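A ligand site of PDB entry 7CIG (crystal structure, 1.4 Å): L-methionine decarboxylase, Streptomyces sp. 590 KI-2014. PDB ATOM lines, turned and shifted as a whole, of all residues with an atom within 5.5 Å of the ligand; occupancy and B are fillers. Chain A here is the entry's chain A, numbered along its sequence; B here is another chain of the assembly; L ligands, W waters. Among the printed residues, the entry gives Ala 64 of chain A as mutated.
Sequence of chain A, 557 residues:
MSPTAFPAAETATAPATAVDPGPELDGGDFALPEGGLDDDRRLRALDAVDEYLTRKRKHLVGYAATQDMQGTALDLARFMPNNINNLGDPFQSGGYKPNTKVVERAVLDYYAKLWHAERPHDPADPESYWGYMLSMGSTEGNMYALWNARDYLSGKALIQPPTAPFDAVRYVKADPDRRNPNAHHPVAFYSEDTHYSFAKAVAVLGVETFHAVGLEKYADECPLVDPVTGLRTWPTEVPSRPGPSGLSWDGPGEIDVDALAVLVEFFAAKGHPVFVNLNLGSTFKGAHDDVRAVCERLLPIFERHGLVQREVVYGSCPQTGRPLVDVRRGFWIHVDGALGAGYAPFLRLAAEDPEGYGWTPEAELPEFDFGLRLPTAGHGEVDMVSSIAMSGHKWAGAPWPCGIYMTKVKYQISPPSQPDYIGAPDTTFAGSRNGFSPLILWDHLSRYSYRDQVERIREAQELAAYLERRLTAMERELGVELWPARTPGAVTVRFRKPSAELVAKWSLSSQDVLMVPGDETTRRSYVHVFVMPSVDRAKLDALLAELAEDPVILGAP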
ATOM      1  N   TYR A  63       6.561  -3.256 -33.433  1.00  0.00           N
ATOM      2  CA  TYR A  63       5.809  -2.729 -32.285  1.00  0.00           C
ATOM      3  C   TYR A  63       4.897  -1.611 -32.768  1.00  0.00           C
ATOM      4  O   TYR A  63       5.198  -0.947 -33.748  1.00  0.00           O
ATOM      5  CB  TYR A  63       6.750  -2.191 -31.191  1.00  0.00           C
ATOM      6  CG  TYR A  63       7.481  -3.295 -30.473  1.00  0.00           C
ATOM      7  CD1 TYR A  63       8.634  -3.869 -30.998  1.00  0.00           C
ATOM      8  CD2 TYR A  63       7.018  -3.778 -29.255  1.00  0.00           C
ATOM      9  CE1 TYR A  63       9.277  -4.910 -30.359  1.00  0.00           C
ATOM     10  CE2 TYR A  63       7.665  -4.803 -28.600  1.00  0.00           C
ATOM     11  CZ  TYR A  63       8.789  -5.375 -29.146  1.00  0.00           C
ATOM     12  OH  TYR A  63       9.403  -6.421 -28.458  1.00  0.00           O
ATOM     13  N   ALA A  64       3.808  -1.394 -32.033  1.00  0.00           N
ATOM     14  CA  ALA A  64       2.832  -0.388 -32.400  1.00  0.00           C
ATOM     15  C   ALA A  64       3.326   0.977 -31.952  1.00  0.00           C
ATOM     16  O   ALA A  64       2.793   1.549 -31.005  1.00  0.00           O
ATOM     17  CB  ALA A  64       1.471  -0.722 -31.796  1.00  0.00           C
ATOM     18  N   ALA A  65       4.331   1.511 -32.643  1.00  0.00           N
ATOM     19  CA  ALA A  65       4.990   2.734 -32.260  1.00  0.00           C
ATOM     20  C   ALA A  65       5.380   3.520 -33.496  1.00  0.00           C
ATOM     21  O   ALA A  65       6.320   3.149 -34.206  1.00  0.00           O
ATOM     22  CB  ALA A  65       6.214   2.414 -31.434  1.00  0.00           C
ATOM     23  N   MET A 136       2.969   8.278 -17.675  1.00  0.00           N
ATOM     24  CA  MET A 136       3.413   6.970 -18.225  1.00  0.00           C
ATOM     25  C   MET A 136       2.627   6.805 -19.570  1.00  0.00           C
ATOM     26  O   MET A 136       2.028   7.753 -20.098  1.00  0.00           O
ATOM     27  CB  MET A 136       3.087   5.807 -17.256  1.00  0.00           C
ATOM     28  CG  MET A 136       3.489   6.044 -15.806  1.00  0.00           C
ATOM     29  SD  MET A 136       3.544   4.654 -14.660  1.00  0.00           S
ATOM     30  CE  MET A 136       1.850   4.066 -14.712  1.00  0.00           C
ATOM     31  N   GLY A 137       2.633   5.597 -20.112  1.00  0.00           N
ATOM     32  CA  GLY A 137       1.738   5.238 -21.200  1.00  0.00           C
ATOM     33  C   GLY A 137       0.367   4.785 -20.738  1.00  0.00           C
ATOM     34  O   GLY A 137      -0.072   5.143 -19.649  1.00  0.00           O
ATOM     35  N   SER A 138      -0.303   3.994 -21.580  1.00  0.00           N
ATOM     36  CA  SER A 138      -1.654   3.531 -21.232  1.00  0.00           C
ATOM     37  C   SER A 138      -1.652   2.681 -19.964  1.00  0.00           C
ATOM     38  O   SER A 138      -2.728   2.486 -19.351  1.00  0.00           O
ATOM     39  CB  SER A 138      -2.339   2.814 -22.393  1.00  0.00           C
ATOM     40  OG  SER A 138      -2.769   3.743 -23.356  1.00  0.00           O
ATOM     41  N   THR A 139      -0.504   2.181 -19.521  1.00  0.00           N
ATOM     42  CA  THR A 139      -0.471   1.493 -18.229  1.00  0.00           C
ATOM     43  C   THR A 139      -1.064   2.392 -17.162  1.00  0.00           C
ATOM     44  O   THR A 139      -1.853   1.920 -16.320  1.00  0.00           O
ATOM     45  CB  THR A 139       0.935   1.046 -17.856  1.00  0.00           C
ATOM     46  OG1 THR A 139       1.421   0.108 -18.843  1.00  0.00           O
ATOM     47  CG2 THR A 139       0.939   0.393 -16.497  1.00  0.00           C
ATOM     48  N   GLU A 140      -0.702   3.669 -17.172  1.00  0.00           N
ATOM     49  CA  GLU A 140      -1.289   4.626 -16.220  1.00  0.00           C
ATOM     50  C   GLU A 140      -2.811   4.769 -16.405  1.00  0.00           C
ATOM     51  O   GLU A 140      -3.561   4.894 -15.443  1.00  0.00           O
ATOM     52  CB  GLU A 140      -0.631   6.020 -16.308  1.00  0.00           C
ATOM     53  CG  GLU A 140      -1.172   7.012 -15.274  1.00  0.00           C
ATOM     54  CD  GLU A 140      -0.540   8.381 -15.358  1.00  0.00           C
ATOM     55  OE1 GLU A 140       0.458   8.571 -16.100  1.00  0.00           O
ATOM     56  OE2 GLU A 140      -1.047   9.306 -14.707  1.00  0.00           O
ATOM     57  N   ASN A 142      -4.984   2.647 -17.789  1.00  0.00           N
ATOM     58  CA  ASN A 142      -5.682   1.428 -17.369  1.00  0.00           C
ATOM     59  C   ASN A 142      -5.675   1.281 -15.856  1.00  0.00           C
ATOM     60  O   ASN A 142      -6.685   0.850 -15.282  1.00  0.00           O
ATOM     61  CB  ASN A 142      -5.088   0.186 -18.003  1.00  0.00           C
ATOM     62  CG  ASN A 142      -5.368   0.093 -19.494  1.00  0.00           C
ATOM     63  OD1 ASN A 142      -6.317   0.678 -20.027  1.00  0.00           O
ATOM     64  ND2 ASN A 142      -4.540  -0.696 -20.186  1.00  0.00           N
ATOM     65  N   HIS A 195      -3.954  -6.951 -22.580  1.00  0.00           N
ATOM     66  CA  HIS A 195      -2.559  -6.607 -22.301  1.00  0.00           C
ATOM     67  C   HIS A 195      -2.202  -6.850 -20.831  1.00  0.00           C
ATOM     68  O   HIS A 195      -3.047  -6.697 -19.938  1.00  0.00           O
ATOM     69  CB  HIS A 195      -2.352  -5.144 -22.726  1.00  0.00           C
ATOM     70  CG  HIS A 195      -0.955  -4.664 -22.560  1.00  0.00           C
ATOM     71  ND1 HIS A 195      -0.550  -3.982 -21.440  1.00  0.00           N
ATOM     72  CD2 HIS A 195       0.120  -4.708 -23.377  1.00  0.00           C
ATOM     73  CE1 HIS A 195       0.733  -3.660 -21.561  1.00  0.00           C
ATOM     74  NE2 HIS A 195       1.165  -4.098 -22.722  1.00  0.00           N
ATOM     75  N   TYR A 196      -0.939  -7.208 -20.607  1.00  0.00           N
ATOM     76  CA  TYR A 196      -0.396  -7.514 -19.257  1.00  0.00           C
ATOM     77  C   TYR A 196      -0.559  -6.435 -18.196  1.00  0.00           C
ATOM     78  O   TYR A 196      -0.537  -6.741 -17.006  1.00  0.00           O
ATOM     79  CB  TYR A 196       1.070  -7.952 -19.366  1.00  0.00           C
ATOM     80  CG  TYR A 196       2.084  -6.863 -19.657  1.00  0.00           C
ATOM     81  CD1 TYR A 196       2.623  -6.074 -18.645  1.00  0.00           C
ATOM     82  CD2 TYR A 196       2.566  -6.657 -20.940  1.00  0.00           C
ATOM     83  CE1 TYR A 196       3.568  -5.081 -18.903  1.00  0.00           C
ATOM     84  CE2 TYR A 196       3.526  -5.688 -21.222  1.00  0.00           C
ATOM     85  CZ  TYR A 196       4.023  -4.898 -20.196  1.00  0.00           C
ATOM     86  OH  TYR A 196       4.963  -3.909 -20.462  1.00  0.00           O
ATOM     87  N   SER A 197      -0.716  -5.175 -18.596  1.00  0.00           N
ATOM     88  CA  SER A 197      -1.039  -4.095 -17.664  1.00  0.00           C
ATOM     89  C   SER A 197      -2.277  -4.326 -16.828  1.00  0.00           C
ATOM     90  O   SER A 197      -2.358  -3.804 -15.727  1.00  0.00           O
ATOM     91  CB  SER A 197      -1.166  -2.708 -18.362  1.00  0.00           C
ATOM     92  OG  SER A 197      -2.183  -2.658 -19.358  1.00  0.00           O
ATOM     93  N   ASN A 279     -10.865  -4.515 -25.487  1.00  0.00           N
ATOM     94  CA  ASN A 279      -9.656  -4.158 -26.224  1.00  0.00           C
ATOM     95  C   ASN A 279      -9.942  -3.574 -27.579  1.00  0.00           C
ATOM     96  O   ASN A 279     -10.555  -4.216 -28.433  1.00  0.00           O
ATOM     97  CB  ASN A 279      -8.747  -5.393 -26.352  1.00  0.00           C
ATOM     98  CG  ASN A 279      -8.492  -6.046 -25.005  1.00  0.00           C
ATOM     99  OD1 ASN A 279      -8.647  -7.284 -24.840  1.00  0.00           O
ATOM    100  ND2 ASN A 279      -8.128  -5.248 -24.050  1.00  0.00           N
ATOM    101  N   GLY A 281      -7.902  -2.657 -30.435  1.00  0.00           N
ATOM    102  CA  GLY A 281      -6.545  -2.766 -31.001  1.00  0.00           C
ATOM    103  C   GLY A 281      -5.673  -3.548 -30.034  1.00  0.00           C
ATOM    104  O   GLY A 281      -4.810  -2.973 -29.342  1.00  0.00           O
ATOM    105  N   SER A 282      -5.906  -4.850 -29.940  1.00  0.00           N
ATOM    106  CA  SER A 282      -5.238  -5.683 -28.966  1.00  0.00           C
ATOM    107  C   SER A 282      -3.725  -5.773 -29.251  1.00  0.00           C
ATOM    108  O   SER A 282      -3.285  -5.579 -30.394  1.00  0.00           O
ATOM    109  CB  SER A 282      -5.884  -7.080 -28.870  1.00  0.00           C
ATOM    110  OG  SER A 282      -5.647  -7.806 -30.049  1.00  0.00           O
ATOM    111  N   THR A 283      -2.957  -6.111 -28.224  1.00  0.00           N
ATOM    112  CA  THR A 283      -1.483  -6.008 -28.347  1.00  0.00           C
ATOM    113  C   THR A 283      -0.882  -6.872 -29.424  1.00  0.00           C
ATOM    114  O   THR A 283      -0.134  -6.357 -30.247  1.00  0.00           O
ATOM    115  CB  THR A 283      -0.819  -6.308 -27.017  1.00  0.00           C
ATOM    116  OG1 THR A 283      -1.385  -5.428 -26.051  1.00  0.00           O
ATOM    117  CG2 THR A 283       0.686  -6.047 -27.073  1.00  0.00           C
ATOM    118  N   ASP A 336      -9.837  -0.177 -23.552  1.00  0.00           N
ATOM    119  CA  ASP A 336      -8.394  -0.060 -23.688  1.00  0.00           C
ATOM    120  C   ASP A 336      -8.066   0.187 -25.153  1.00  0.00           C
ATOM    121  O   ASP A 336      -7.928  -0.735 -25.962  1.00  0.00           O
ATOM    122  CB  ASP A 336      -7.659  -1.302 -23.191  1.00  0.00           C
ATOM    123  CG  ASP A 336      -6.147  -1.144 -23.237  1.00  0.00           C
ATOM    124  OD1 ASP A 336      -5.695  -0.087 -23.761  1.00  0.00           O
ATOM    125  OD2 ASP A 336      -5.457  -2.071 -22.756  1.00  0.00           O
ATOM    126  N   ALA A 338      -5.427   1.884 -26.094  1.00  0.00           N
ATOM    127  CA  ALA A 338      -3.996   2.267 -26.138  1.00  0.00           C
ATOM    128  C   ALA A 338      -3.544   2.545 -27.585  1.00  0.00           C
ATOM    129  O   ALA A 338      -2.986   3.611 -27.908  1.00  0.00           O
ATOM    130  CB  ALA A 338      -3.139   1.192 -25.508  1.00  0.00           C
ATOM    131  N   LEU A 339      -3.789   1.575 -28.451  1.00  0.00           N
ATOM    132  CA  LEU A 339      -3.531   1.724 -29.856  1.00  0.00           C
ATOM    133  C   LEU A 339      -4.748   2.298 -30.569  1.00  0.00           C
ATOM    134  O   LEU A 339      -4.700   3.349 -31.210  1.00  0.00           O
ATOM    135  CB  LEU A 339      -3.138   0.360 -30.448  1.00  0.00           C
ATOM    136  CG  LEU A 339      -3.021   0.309 -31.967  1.00  0.00           C
ATOM    137  CD1 LEU A 339      -1.986   1.276 -32.498  1.00  0.00           C
ATOM    138  CD2 LEU A 339      -2.701  -1.097 -32.407  1.00  0.00           C
ATOM    139  N   SER A 391      -2.723   5.555 -25.864  1.00  0.00           N
ATOM    140  CA  SER A 391      -1.291   5.914 -25.803  1.00  0.00           C
ATOM    141  C   SER A 391      -0.965   6.863 -26.937  1.00  0.00           C
ATOM    142  O   SER A 391      -1.240   6.550 -28.103  1.00  0.00           O
ATOM    143  CB  SER A 391      -0.425   4.655 -25.954  1.00  0.00           C
ATOM    144  OG  SER A 391      -0.586   3.743 -24.887  1.00  0.00           O
ATOM    145  N   HIS A 393       2.187   7.664 -27.822  1.00  0.00           N
ATOM    146  CA  HIS A 393       3.388   7.104 -28.466  1.00  0.00           C
ATOM    147  C   HIS A 393       3.104   5.895 -29.351  1.00  0.00           C
ATOM    148  O   HIS A 393       4.033   5.354 -29.951  1.00  0.00           O
ATOM    149  CB  HIS A 393       4.486   6.729 -27.433  1.00  0.00           C
ATOM    150  CG  HIS A 393       3.947   5.863 -26.355  1.00  0.00           C
ATOM    151  ND1 HIS A 393       4.361   4.567 -26.086  1.00  0.00           N
ATOM    152  CD2 HIS A 393       2.938   6.114 -25.495  1.00  0.00           C
ATOM    153  CE1 HIS A 393       3.618   4.082 -25.111  1.00  0.00           C
ATOM    154  NE2 HIS A 393       2.750   5.003 -24.740  1.00  0.00           N
ATOM    155  N   LYS A 394       1.846   5.453 -29.433  1.00  0.00           N
ATOM    156  CA  LYS A 394       1.467   4.394 -30.360  1.00  0.00           C
ATOM    157  C   LYS A 394       1.077   5.018 -31.717  1.00  0.00           C
ATOM    158  O   LYS A 394       1.959   5.302 -32.550  1.00  0.00           O
ATOM    159  CB  LYS A 394       0.429   3.440 -29.728  1.00  0.00           C
ATOM    160  CG  LYS A 394       1.048   2.653 -28.586  1.00  0.00           C
ATOM    161  CD  LYS A 394       0.206   1.526 -27.957  1.00  0.00           C
ATOM    162  CE  LYS A 394       1.108   0.534 -27.191  1.00  0.00           C
ATOM    163  NZ  LYS A 394       0.603  -0.498 -26.195  1.00  0.00           N
ATOM    164  N   PRO A 401       6.672   7.773 -23.518  1.00  0.00           N
ATOM    165  CA  PRO A 401       5.319   7.346 -23.280  1.00  0.00           C
ATOM    166  C   PRO A 401       4.435   8.457 -22.761  1.00  0.00           C
ATOM    167  O   PRO A 401       4.841   9.267 -21.946  1.00  0.00           O
ATOM    168  CB  PRO A 401       5.462   6.240 -22.239  1.00  0.00           C
ATOM    169  CG  PRO A 401       6.837   5.670 -22.534  1.00  0.00           C
ATOM    170  CD  PRO A 401       7.641   6.903 -22.810  1.00  0.00           C
ATOM    171  N   CYS A 402       3.217   8.507 -23.303  1.00  0.00           N
ATOM    172  CA  CYS A 402       2.219   9.487 -22.940  1.00  0.00           C
ATOM    173  C   CYS A 402       0.851   8.952 -23.375  1.00  0.00           C
ATOM    174  O   CYS A 402       0.730   7.875 -23.939  1.00  0.00           O
ATOM    175  CB  CYS A 402       2.520  10.841 -23.597  1.00  0.00           C
ATOM    176  SG  CYS A 402       2.463  10.782 -25.403  1.00  0.00           S
ATOM    177  N   SER A 509       8.457  -8.031 -32.589  1.00  0.00           N
ATOM    178  CA  SER A 509       7.956  -8.500 -31.313  1.00  0.00           C
ATOM    179  C   SER A 509       7.550  -9.964 -31.464  1.00  0.00           C
ATOM    180  O   SER A 509       6.997 -10.358 -32.477  1.00  0.00           O
ATOM    181  CB  SER A 509       6.742  -7.658 -30.888  1.00  0.00           C
ATOM    182  OG  SER A 509       6.225  -8.086 -29.635  1.00  0.00           O
ATOM    183  N   ASN B  85      11.742   3.603 -26.141  1.00  0.00           N
ATOM    184  CA  ASN B  85      10.915   2.906 -25.168  1.00  0.00           C
ATOM    185  C   ASN B  85      11.764   1.921 -24.422  1.00  0.00           C
ATOM    186  O   ASN B  85      12.289   0.994 -25.030  1.00  0.00           O
ATOM    187  CB  ASN B  85       9.758   2.226 -25.894  1.00  0.00           C
ATOM    188  CG  ASN B  85       8.659   1.799 -24.958  1.00  0.00           C
ATOM    189  OD1 ASN B  85       8.883   1.504 -23.779  1.00  0.00           O
ATOM    190  ND2 ASN B  85       7.454   1.697 -25.494  1.00  0.00           N
ATOM    191  N   LEU B  87      10.911  -0.382 -22.398  1.00  0.00           N
ATOM    192  CA  LEU B  87       9.950  -1.397 -22.064  1.00  0.00           C
ATOM    193  C   LEU B  87      10.628  -2.586 -21.398  1.00  0.00           C
ATOM    194  O   LEU B  87      11.566  -3.150 -21.965  1.00  0.00           O
ATOM    195  CB  LEU B  87       9.340  -1.851 -23.403  1.00  0.00           C
ATOM    196  CG  LEU B  87       8.160  -2.788 -23.410  1.00  0.00           C
ATOM    197  CD1 LEU B  87       6.967  -2.096 -22.788  1.00  0.00           C
ATOM    198  CD2 LEU B  87       7.858  -3.165 -24.854  1.00  0.00           C
ATOM    199  N   TYR B  96      12.193  -4.413 -28.134  1.00  0.00           N
ATOM    200  CA  TYR B  96      12.039  -3.031 -28.627  1.00  0.00           C
ATOM    201  C   TYR B  96      13.436  -2.422 -28.661  1.00  0.00           C
ATOM    202  O   TYR B  96      13.919  -1.888 -27.648  1.00  0.00           O
ATOM    203  CB  TYR B  96      11.066  -2.231 -27.751  1.00  0.00           C
ATOM    204  CG  TYR B  96      10.593  -0.929 -28.339  1.00  0.00           C
ATOM    205  CD1 TYR B  96      11.424   0.199 -28.406  1.00  0.00           C
ATOM    206  CD2 TYR B  96       9.298  -0.790 -28.837  1.00  0.00           C
ATOM    207  CE1 TYR B  96      10.986   1.391 -28.935  1.00  0.00           C
ATOM    208  CE2 TYR B  96       8.839   0.395 -29.360  1.00  0.00           C
ATOM    209  CZ  TYR B  96       9.690   1.502 -29.443  1.00  0.00           C
ATOM    210  OH  TYR B  96       9.273   2.712 -29.955  1.00  0.00           O
ATOM    211  N   TYR B 421       5.878 -10.600 -25.362  1.00  0.00           N
ATOM    212  CA  TYR B 421       5.972  -9.613 -26.436  1.00  0.00           C
ATOM    213  C   TYR B 421       6.873  -8.401 -26.159  1.00  0.00           C
ATOM    214  O   TYR B 421       7.205  -7.660 -27.081  1.00  0.00           O
ATOM    215  CB  TYR B 421       4.576  -9.171 -26.944  1.00  0.00           C
ATOM    216  CG  TYR B 421       3.466  -9.018 -25.910  1.00  0.00           C
ATOM    217  CD1 TYR B 421       2.469  -9.992 -25.771  1.00  0.00           C
ATOM    218  CD2 TYR B 421       3.384  -7.893 -25.100  1.00  0.00           C
ATOM    219  CE1 TYR B 421       1.439  -9.863 -24.846  1.00  0.00           C
ATOM    220  CE2 TYR B 421       2.369  -7.737 -24.172  1.00  0.00           C
ATOM    221  CZ  TYR B 421       1.390  -8.721 -24.041  1.00  0.00           C
ATOM    222  OH  TYR B 421       0.371  -8.581 -23.129  1.00  0.00           O
ATOM    223  N   ILE B 422       7.292  -8.223 -24.915  1.00  0.00           N
ATOM    224  CA  ILE B 422       8.260  -7.172 -24.598  1.00  0.00           C
ATOM    225  C   ILE B 422       9.720  -7.690 -24.503  1.00  0.00           C
ATOM    226  O   ILE B 422      10.660  -6.874 -24.545  1.00  0.00           O
ATOM    227  CB  ILE B 422       7.796  -6.362 -23.361  1.00  0.00           C
ATOM    228  CG1 ILE B 422       7.988  -7.111 -22.039  1.00  0.00           C
ATOM    229  CG2 ILE B 422       6.327  -5.955 -23.511  1.00  0.00           C
ATOM    230  CD1 ILE B 422       8.126  -6.176 -20.858  1.00  0.00           C
ATOM    231  N   ALA B 430       5.379   1.199 -14.472  1.00  0.00           N
ATOM    232  CA  ALA B 430       5.073   1.484 -15.894  1.00  0.00           C
ATOM    233  C   ALA B 430       5.228   0.257 -16.779  1.00  0.00           C
ATOM    234  O   ALA B 430       5.883  -0.706 -16.387  1.00  0.00           O
ATOM    235  CB  ALA B 430       5.963   2.593 -16.453  1.00  0.00           C
ATOM    236  N   GLY B 431       4.601   0.330 -17.948  1.00  0.00           N
ATOM    237  CA  GLY B 431       4.705  -0.652 -19.020  1.00  0.00           C
ATOM    238  C   GLY B 431       5.747  -0.138 -19.990  1.00  0.00           C
ATOM    239  O   GLY B 431       6.929  -0.275 -19.721  1.00  0.00           O
ATOM    240  N   SER B 432       5.323   0.524 -21.081  1.00  0.00           N
ATOM    241  CA  SER B 432       6.271   1.376 -21.795  1.00  0.00           C
ATOM    242  C   SER B 432       6.959   2.275 -20.784  1.00  0.00           C
ATOM    243  O   SER B 432       6.326   2.770 -19.860  1.00  0.00           O
ATOM    244  CB  SER B 432       5.567   2.264 -22.827  1.00  0.00           C
ATOM    245  OG  SER B 432       5.038   1.503 -23.900  1.00  0.00           O
HETATM  246  O1  LIG L   1       2.989   0.410 -22.742  1.00  0.00           O
HETATM  247  P1  LIG L   1       1.907   1.445 -22.338  1.00  0.00           P
HETATM  248  O2  LIG L   1       1.952   2.691 -23.186  1.00  0.00           O
HETATM  249  O3  LIG L   1       1.953   1.691 -20.861  1.00  0.00           O
HETATM  250  O4  LIG L   1       0.497   0.785 -22.744  1.00  0.00           O
HETATM  251  C1  LIG L   1       0.169  -0.463 -22.296  1.00  0.00           C
HETATM  252  C2  LIG L   1      -0.745  -1.059 -23.247  1.00  0.00           C
HETATM  253  C3  LIG L   1      -2.043  -1.305 -22.811  1.00  0.00           C
HETATM  254  N1  LIG L   1      -3.005  -1.899 -23.677  1.00  0.00           N
HETATM  255  C4  LIG L   1      -2.698  -2.254 -24.915  1.00  0.00           C
HETATM  256  C5  LIG L   1      -3.779  -2.877 -25.763  1.00  0.00           C
HETATM  257  C6  LIG L   1      -1.407  -2.038 -25.382  1.00  0.00           C
HETATM  258  O5  LIG L   1      -1.106  -2.439 -26.618  1.00  0.00           O
HETATM  259  C7  LIG L   1      -0.422  -1.430 -24.579  1.00  0.00           C
HETATM  260  C8  LIG L   1       0.857  -1.207 -25.096  1.00  0.00           C
HETATM  261  N2  LIG L   1       1.538  -2.297 -25.777  1.00  0.00           N
HETATM  262  C9  LIG L   1       2.920  -2.335 -26.279  1.00  0.00           C
HETATM  263  C10 LIG L   1       3.451  -3.700 -25.881  1.00  0.00           C
HETATM  264  O6  LIG L   1       3.051  -4.282 -24.865  1.00  0.00           O
HETATM  265  O7  LIG L   1       4.450  -4.158 -26.679  1.00  0.00           O
HETATM  266  C11 LIG L   1       4.487  -5.539 -27.111  1.00  0.00           C
HETATM  267  C12 LIG L   1       3.817  -1.226 -25.707  1.00  0.00           C
HETATM  268  C13 LIG L   1       5.028  -1.130 -26.664  1.00  0.00           C
HETATM  269  S1  LIG L   1       4.632  -0.375 -28.285  1.00  0.00           S
HETATM  270  C14 LIG L   1       4.654   1.394 -28.046  1.00  0.00           C
HETATM  271  O   HOH W   1      -1.902  -2.442 -29.112  1.00  0.00           O
HETATM  272  O   HOH W   2       3.423  -2.244 -21.821  1.00  0.00           O
HETATM  273  O   HOH W   3       7.128   3.276 -28.008  1.00  0.00           O
HETATM  274  O   HOH W   4      -4.820  -6.152 -25.806  1.00  0.00           O
HETATM  275  O   HOH W   5      -5.386  -0.710 -27.844  1.00  0.00           O
HETATM  276  O   HOH W   6       3.710   2.932 -19.281  1.00  0.00           O
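NE2 of His 393 is in hydrogen-bond range of O2 of the ligand, at 2.9 Å.
OG of Ser 391 lies within hydrogen-bond range of O2 of the ligand (3.2 Å).
An oxygen (O6) of the ligand sits at hydrogen-bond distance from a ring nitrogen (NE2) of His 195, at 2.9 Å.
N1 of the ligand is in hydrogen-bond range of OD2 of Asp 336 (2.6 Å).
The side-chain hydroxyl of Thr 283 sits at hydrogen-bond distance from an oxygen (O5) of the ligand (3.1 Å).
The side-chain hydroxyl (OG) of Ser 432 of chain B is in hydrogen-bond range of an oxygen (O1) of the ligand, at 2.6 Å.
The side-chain hydroxyl of Thr 139 sits at hydrogen-bond distance from an oxygen (O3) of the ligand (2.6 Å).
The side-chain amino group (NZ) of Lys 394 is bonded to a carbon (C8) of the ligand (1.3 Å).
The backbone NH (N) of Thr 139 is in hydrogen-bond range of an oxygen (O3) of the ligand, 2.8 Å away.
An oxygen (O2) of the ligand is in hydrogen-bond range of the backbone NH of Ser 138 (3.1 Å).
N of Ser 432 of chain B sits at hydrogen-bond distance from O1 of the ligand, 2.9 Å away.
The side-chain hydroxyl of Thr 139 is in hydrogen-bond range of the backbone NH of Gly 431 of chain B.
OD1 of Asp 336 lies within hydrogen-bond range of N of Ala 338 (3.1 Å).
A ring nitrogen (ND1) of His 195 lies within hydrogen-bond range of the side-chain hydroxyl of Ser 197 (3.0 Å).
The side-chain hydroxyl (OG) of Ser 432 of chain B is in hydrogen-bond range of the side-chain amide nitrogen (ND2) of Asn 85 of chain B (2.9 Å).
The backbone NH (N) of Ser 391 sits at hydrogen-bond distance from the backbone carbonyl oxygen (O) of Ala 338 (2.8 Å).
OG of Ser 197 sits at hydrogen-bond distance from ND2 of Asn 142.
The backbone NH (N) of Tyr 196 lies within hydrogen-bond range of the side-chain hydroxyl (OH) of Tyr 421 of chain B (3.2 Å).
The side-chain amide nitrogen (ND2) of Asn 142 sits at hydrogen-bond distance from the side-chain carboxylate (OD2) of Asp 336.
Merely in contact with the ligand: Gly 137 (3.2 Å), Tyr 421 of chain B (3.3 Å), Ala 64 (3.5 Å), Ala 338 (3.5 Å), Tyr 63 (3.6 Å), Asn 142 (3.7 Å), Ser 197 (3.7 Å), Gly 281 (3.7 Å), Asn 85 of chain B (3.8 Å), Ala 65 (3.9 Å), Ile 422 of chain B (3.9 Å), Leu 87 of chain B (3.9 Å), Tyr 196 (3.9 Å), Gly 431 of chain B (3.9 Å) and Ser 509 (3.98 Å).
Hydrophobic or aromatic side chains within 4 Å of the ligand: Tyr 63, Ala 65, His 195, Tyr 196, Ala 338, His 393, Leu 87 of chain B, Tyr 421 of chain B and Ile 422 of chain B.
Of the 33 residues printed, 24 come within 4 Å of the ligand.
The nearest printed residue that does not touch the ligand is Tyr 96 of chain B (4.4 Å).
Water W1 lies within hydrogen-bond range of O5 of the ligand (2.6 Å) and O of Gly 281 (3.0 Å).
Water W6 lies within hydrogen-bond range of O3 of the ligand (2.7 Å), O of Ser 432 of chain B (2.7 Å), N of Gly 137 (3.0 Å) and N of Gly 431 of chain B (3.1 Å).
Water W2 lies within hydrogen-bond range of OH of Tyr 196 (2.6 Å), O1 of the ligand (2.8 Å), NE2 of His 195 (3.1 Å) and N of Ser 432 of chain B (3.4 Å).
Water W3 bridges OH of Tyr 96 of chain B (3.0 Å) and ND2 of Asn 85 of chain B (3.0 Å).
Water W5 lies within hydrogen-bond range of the backbone carbonyl oxygen (O) of Gly 281 (2.8 Å), the backbone NH (N) of Leu 339 (2.9 Å), the backbone NH (N) of Ala 338 (3.1 Å) and the backbone carbonyl oxygen (O) of Asp 336 (3.2 Å).
Water W4 bridges the backbone NH (N) of Thr 283 (3.1 Å) and the backbone NH (N) of His 195 (3.4 Å).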
